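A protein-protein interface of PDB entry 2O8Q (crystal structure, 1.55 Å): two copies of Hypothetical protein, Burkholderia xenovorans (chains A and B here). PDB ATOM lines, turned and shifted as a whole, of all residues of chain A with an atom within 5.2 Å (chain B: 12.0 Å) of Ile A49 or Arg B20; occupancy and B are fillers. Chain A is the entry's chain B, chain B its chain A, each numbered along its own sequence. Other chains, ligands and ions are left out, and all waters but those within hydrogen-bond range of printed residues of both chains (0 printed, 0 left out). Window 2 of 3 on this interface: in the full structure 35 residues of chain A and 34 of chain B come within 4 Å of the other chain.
Of the 10 printed residues of chain A, 5 touch a printed residue of chain B. Printed residues of chain A that touch a printed residue of chain B: Phe A26, Glu A27, Tyr A28, Arg A47 and Ile A49. Hydrophobic or aromatic side chains of chain A within 4 Å of the printed part of chain B: Tyr A28 and Ile A49. Printed residues of chain B that touch a printed residue of chain A: Gly B15, Gly B17, Phe B18, Asp B19 and Arg B20. Hydrophobic or aromatic side chains of chain B within 4 Å of the printed part of chain A: Phe B18. Among the printed residues, 10 pairs touch across the chains. Among the printed residues, no Asp or Glu carboxylate lies within 4 Å of a Lys or Arg side-chain nitrogen of the other chain.
NH1 of Arg A47 is in hydrogen-bond range of O of Gly B15 (3.2 Å). The backbone NH (N) of Asp B19 sits at hydrogen-bond distance from the backbone carbonyl oxygen (O) of Tyr A28 (2.8 Å).
No position is printed for both chains. Of the 10 pairs that touch across the chains among the printed residues, none has its exchanged pair printed and touching as well.
Phe A25 touches none of the printed residues of chain B. Glu A27 touches three residues of chain B. Of the printed residues of chain B, Tyr A28 touches Gly B17, Phe B18 and Asp B19. Of the printed residues of chain B, Arg A47 touches Gly B15 (3.2 Å) and Phe B18 (3.5 Å). Ile A49 touches one residue of chain B. No residue of chain B comes within 4 Å of Pro A50. Ser B16 touches none of the printed residues of chain A. Of the printed residues of chain A, Phe B18 touches Glu A27 (3.6 Å), Tyr A28 (3.3 Å) and Arg A47 (3.5 Å). Printed residues of chain A within 4 Å of Asp B19: Glu A27 (3.4 Å) and Tyr A28 (2.8 Å).
The backbone carbonyl oxygen of Phe A25 lies within hydrogen-bond range of the backbone NH of Ile A49 (3.1 Å). OE2 of Glu A27 is in salt-bridge range of NH2 of Arg A47.
Among the printed residues, merely in contact across the chains: Phe A26 with Arg B20 (3.9 Å), Glu A27 with Phe B18 (3.6 Å), Glu A27 with Asp B19 (3.4 Å), Glu A27 with Arg B20 (3.8 Å), Tyr A28 with Gly B17 (3.8 Å), Tyr A28 with Phe B18 (3.3 Å), Arg A47 with Phe B18 (3.5 Å) and Ile A49 with Arg B20 (3.7 Å).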
ATOM      1  N   GLU A  24      -6.206  28.762  25.664  1.00  0.00           N
ATOM      2  CA  GLU A  24      -6.040  29.025  24.248  1.00  0.00           C
ATOM      3  C   GLU A  24      -7.148  28.401  23.429  1.00  0.00           C
ATOM      4  O   GLU A  24      -7.614  28.984  22.448  1.00  0.00           O
ATOM      5  CB  GLU A  24      -4.685  28.481  23.764  1.00  0.00           C
ATOM      6  CG  GLU A  24      -4.419  28.668  22.271  1.00  0.00           C
ATOM      7  CD  GLU A  24      -2.938  28.824  21.947  1.00  0.00           C
ATOM      8  OE1 GLU A  24      -2.117  28.073  22.524  1.00  0.00           O
ATOM      9  OE2 GLU A  24      -2.600  29.697  21.115  1.00  0.00           O
ATOM     10  N   PHE A  25      -7.559  27.198  23.810  1.00  0.00           N
ATOM     11  CA  PHE A  25      -8.463  26.432  22.986  1.00  0.00           C
ATOM     12  C   PHE A  25      -9.930  26.514  23.471  1.00  0.00           C
ATOM     13  O   PHE A  25     -10.865  26.274  22.697  1.00  0.00           O
ATOM     14  CB  PHE A  25      -7.960  24.977  22.904  1.00  0.00           C
ATOM     15  CG  PHE A  25      -6.618  24.834  22.203  1.00  0.00           C
ATOM     16  CD1 PHE A  25      -6.473  25.195  20.866  1.00  0.00           C
ATOM     17  CD2 PHE A  25      -5.507  24.348  22.883  1.00  0.00           C
ATOM     18  CE1 PHE A  25      -5.238  25.079  20.216  1.00  0.00           C
ATOM     19  CE2 PHE A  25      -4.266  24.226  22.229  1.00  0.00           C
ATOM     20  CZ  PHE A  25      -4.143  24.593  20.900  1.00  0.00           C
ATOM     21  N   PHE A  26     -10.115  26.863  24.747  1.00  0.00           N
ATOM     22  CA  PHE A  26     -11.440  26.817  25.381  1.00  0.00           C
ATOM     23  C   PHE A  26     -11.635  28.006  26.313  1.00  0.00           C
ATOM     24  O   PHE A  26     -10.684  28.628  26.724  1.00  0.00           O
ATOM     25  CB  PHE A  26     -11.651  25.495  26.148  1.00  0.00           C
ATOM     26  CG  PHE A  26     -11.634  24.281  25.263  1.00  0.00           C
ATOM     27  CD1 PHE A  26     -12.781  23.886  24.598  1.00  0.00           C
ATOM     28  CD2 PHE A  26     -10.458  23.597  25.031  1.00  0.00           C
ATOM     29  CE1 PHE A  26     -12.764  22.796  23.748  1.00  0.00           C
ATOM     30  CE2 PHE A  26     -10.441  22.541  24.190  1.00  0.00           C
ATOM     31  CZ  PHE A  26     -11.591  22.131  23.551  1.00  0.00           C
ATOM     32  N   GLU A  27     -12.896  28.351  26.566  1.00  0.00           N
ATOM     33  CA  GLU A  27     -13.269  29.385  27.540  1.00  0.00           C
ATOM     34  C   GLU A  27     -14.310  28.779  28.473  1.00  0.00           C
ATOM     35  O   GLU A  27     -14.957  27.778  28.124  1.00  0.00           O
ATOM     36  CB  GLU A  27     -13.769  30.667  26.883  1.00  0.00           C
ATOM     37  CG  GLU A  27     -14.990  30.510  26.012  1.00  0.00           C
ATOM     38  CD  GLU A  27     -15.318  31.740  25.216  1.00  0.00           C
ATOM     39  OE1 GLU A  27     -14.664  32.781  25.385  1.00  0.00           O
ATOM     40  OE2 GLU A  27     -16.253  31.644  24.409  1.00  0.00           O
ATOM     41  N   TYR A  28     -14.412  29.351  29.680  1.00  0.00           N
ATOM     42  CA  TYR A  28     -15.097  28.714  30.812  1.00  0.00           C
ATOM     43  C   TYR A  28     -16.035  29.694  31.483  1.00  0.00           C
ATOM     44  O   TYR A  28     -15.705  30.871  31.700  1.00  0.00           O
ATOM     45  CB  TYR A  28     -14.110  28.164  31.867  1.00  0.00           C
ATOM     46  CG  TYR A  28     -13.147  27.108  31.316  1.00  0.00           C
ATOM     47  CD1 TYR A  28     -12.147  27.521  30.452  1.00  0.00           C
ATOM     48  CD2 TYR A  28     -13.240  25.754  31.621  1.00  0.00           C
ATOM     49  CE1 TYR A  28     -11.270  26.671  29.883  1.00  0.00           C
ATOM     50  CE2 TYR A  28     -12.303  24.839  31.026  1.00  0.00           C
ATOM     51  CZ  TYR A  28     -11.336  25.365  30.135  1.00  0.00           C
ATOM     52  OH  TYR A  28     -10.355  24.620  29.490  1.00  0.00           O
ATOM     53  N   ARG A  47     -16.611  26.083  26.575  1.00  0.00           N
ATOM     54  CA  ARG A  47     -16.999  26.318  25.200  1.00  0.00           C
ATOM     55  C   ARG A  47     -15.756  26.359  24.318  1.00  0.00           C
ATOM     56  O   ARG A  47     -14.741  26.950  24.682  1.00  0.00           O
ATOM     57  CB  ARG A  47     -17.765  27.632  25.107  1.00  0.00           C
ATOM     58  CG  ARG A  47     -18.510  27.938  23.864  1.00  0.00           C
ATOM     59  CD  ARG A  47     -19.432  29.148  24.145  1.00  0.00           C
ATOM     60  NE  ARG A  47     -18.701  30.411  24.401  1.00  0.00           N
ATOM     61  CZ  ARG A  47     -19.308  31.596  24.591  1.00  0.00           C
ATOM     62  NH1 ARG A  47     -20.631  31.646  24.637  1.00  0.00           N
ATOM     63  NH2 ARG A  47     -18.607  32.707  24.783  1.00  0.00           N
ATOM     64  N   ALA A  48     -15.848  25.733  23.152  1.00  0.00           N
ATOM     65  CA  ALA A  48     -14.786  25.820  22.145  1.00  0.00           C
ATOM     66  C   ALA A  48     -14.595  27.266  21.650  1.00  0.00           C
ATOM     67  O   ALA A  48     -15.567  27.988  21.487  1.00  0.00           O
ATOM     68  CB  ALA A  48     -15.133  24.915  21.006  1.00  0.00           C
ATOM     69  N   ILE A  49     -13.338  27.658  21.426  1.00  0.00           N
ATOM     70  CA  ILE A  49     -12.979  28.877  20.698  1.00  0.00           C
ATOM     71  C   ILE A  49     -12.753  28.395  19.263  1.00  0.00           C
ATOM     72  O   ILE A  49     -11.838  27.590  19.062  1.00  0.00           O
ATOM     73  CB  ILE A  49     -11.649  29.434  21.238  1.00  0.00           C
ATOM     74  CG1 ILE A  49     -11.791  29.895  22.682  1.00  0.00           C
ATOM     75  CG2 ILE A  49     -11.159  30.599  20.349  1.00  0.00           C
ATOM     76  CD1 ILE A  49     -10.511  30.437  23.262  1.00  0.00           C
ATOM     77  N   PRO A  50     -13.576  28.867  18.262  1.00  0.00           N
ATOM     78  CA  PRO A  50     -13.471  28.397  16.847  1.00  0.00           C
ATOM     79  C   PRO A  50     -12.143  28.793  16.209  1.00  0.00           C
ATOM     80  O   PRO A  50     -11.607  29.839  16.588  1.00  0.00           O
ATOM     81  CB  PRO A  50     -14.631  29.128  16.105  1.00  0.00           C
ATOM     82  CG  PRO A  50     -15.455  29.799  17.156  1.00  0.00           C
ATOM     83  CD  PRO A  50     -14.631  29.896  18.424  1.00  0.00           C
ATOM     84  N   ASP A 108     -16.963  23.109  16.433  1.00  0.00           N
ATOM     85  CA  ASP A 108     -16.665  24.479  16.766  1.00  0.00           C
ATOM     86  C   ASP A 108     -17.627  25.178  17.704  1.00  0.00           C
ATOM     87  O   ASP A 108     -17.307  26.193  18.327  1.00  0.00           O
ATOM     88  CB  ASP A 108     -16.745  25.280  15.492  1.00  0.00           C
ATOM     89  CG  ASP A 108     -15.520  25.086  14.530  1.00  0.00           C
ATOM     90  OD1 ASP A 108     -14.556  24.381  14.895  1.00  0.00           O
ATOM     91  OD2 ASP A 108     -15.531  25.678  13.458  1.00  0.00           O
ATOM     92  N   GLY B  15     -24.571  35.987  25.737  1.00  0.00           N
ATOM     93  CA  GLY B  15     -23.522  34.989  25.445  1.00  0.00           C
ATOM     94  C   GLY B  15     -22.167  35.272  26.085  1.00  0.00           C
ATOM     95  O   GLY B  15     -21.201  34.516  25.899  1.00  0.00           O
ATOM     96  N   SER B  16     -22.103  36.357  26.845  1.00  0.00           N
ATOM     97  CA  SER B  16     -20.961  36.663  27.676  1.00  0.00           C
ATOM     98  C   SER B  16     -20.909  35.722  28.902  1.00  0.00           C
ATOM     99  O   SER B  16     -21.645  34.726  28.976  1.00  0.00           O
ATOM    100  CB  SER B  16     -21.068  38.114  28.125  1.00  0.00           C
ATOM    101  OG  SER B  16     -22.209  38.300  28.940  1.00  0.00           O
ATOM    102  N   GLY B  17     -20.041  36.044  29.855  1.00  0.00           N
ATOM    103  CA  GLY B  17     -19.859  35.228  31.050  1.00  0.00           C
ATOM    104  C   GLY B  17     -18.776  34.169  30.948  1.00  0.00           C
ATOM    105  O   GLY B  17     -18.551  33.448  31.907  1.00  0.00           O
ATOM    106  N   PHE B  18     -18.112  34.051  29.801  1.00  0.00           N
ATOM    107  CA  PHE B  18     -17.028  33.104  29.644  1.00  0.00           C
ATOM    108  C   PHE B  18     -15.694  33.800  29.732  1.00  0.00           C
ATOM    109  O   PHE B  18     -15.514  34.927  29.242  1.00  0.00           O
ATOM    110  CB  PHE B  18     -17.113  32.368  28.314  1.00  0.00           C
ATOM    111  CG  PHE B  18     -18.220  31.363  28.259  1.00  0.00           C
ATOM    112  CD1 PHE B  18     -19.536  31.769  28.085  1.00  0.00           C
ATOM    113  CD2 PHE B  18     -17.936  30.019  28.380  1.00  0.00           C
ATOM    114  CE1 PHE B  18     -20.557  30.843  28.000  1.00  0.00           C
ATOM    115  CE2 PHE B  18     -18.942  29.070  28.304  1.00  0.00           C
ATOM    116  CZ  PHE B  18     -20.273  29.498  28.128  1.00  0.00           C
ATOM    117  N   ASP B  19     -14.755  33.103  30.349  1.00  0.00           N
ATOM    118  CA  ASP B  19     -13.405  33.610  30.581  1.00  0.00           C
ATOM    119  C   ASP B  19     -12.414  32.647  29.879  1.00  0.00           C
ATOM    120  O   ASP B  19     -12.412  31.438  30.106  1.00  0.00           O
ATOM    121  CB  ASP B  19     -13.161  33.677  32.094  1.00  0.00           C
ATOM    122  CG  ASP B  19     -12.283  34.827  32.493  1.00  0.00           C
ATOM    123  OD1 ASP B  19     -12.616  35.992  32.141  1.00  0.00           O
ATOM    124  OD2 ASP B  19     -11.258  34.559  33.165  1.00  0.00           O
ATOM    125  N   ARG B  20     -11.557  33.208  29.020  1.00  0.00           N
ATOM    126  CA  ARG B  20     -10.669  32.398  28.175  1.00  0.00           C
ATOM    127  C   ARG B  20      -9.602  31.660  28.992  1.00  0.00           C
ATOM    128  O   ARG B  20      -8.707  32.274  29.564  1.00  0.00           O
ATOM    129  CB  ARG B  20     -10.024  33.283  27.104  1.00  0.00           C
ATOM    130  CG  ARG B  20      -9.218  32.528  26.055  1.00  0.00           C
ATOM    131  CD  ARG B  20      -8.591  33.448  24.997  1.00  0.00           C
ATOM    132  NE  ARG B  20      -8.175  34.778  25.497  1.00  0.00           N
ATOM    133  CZ  ARG B  20      -7.113  35.481  25.066  1.00  0.00           C
ATOM    134  NH1 ARG B  20      -6.297  35.006  24.124  1.00  0.00           N
ATOM    135  NH2 ARG B  20      -6.852  36.680  25.592  1.00  0.00           N
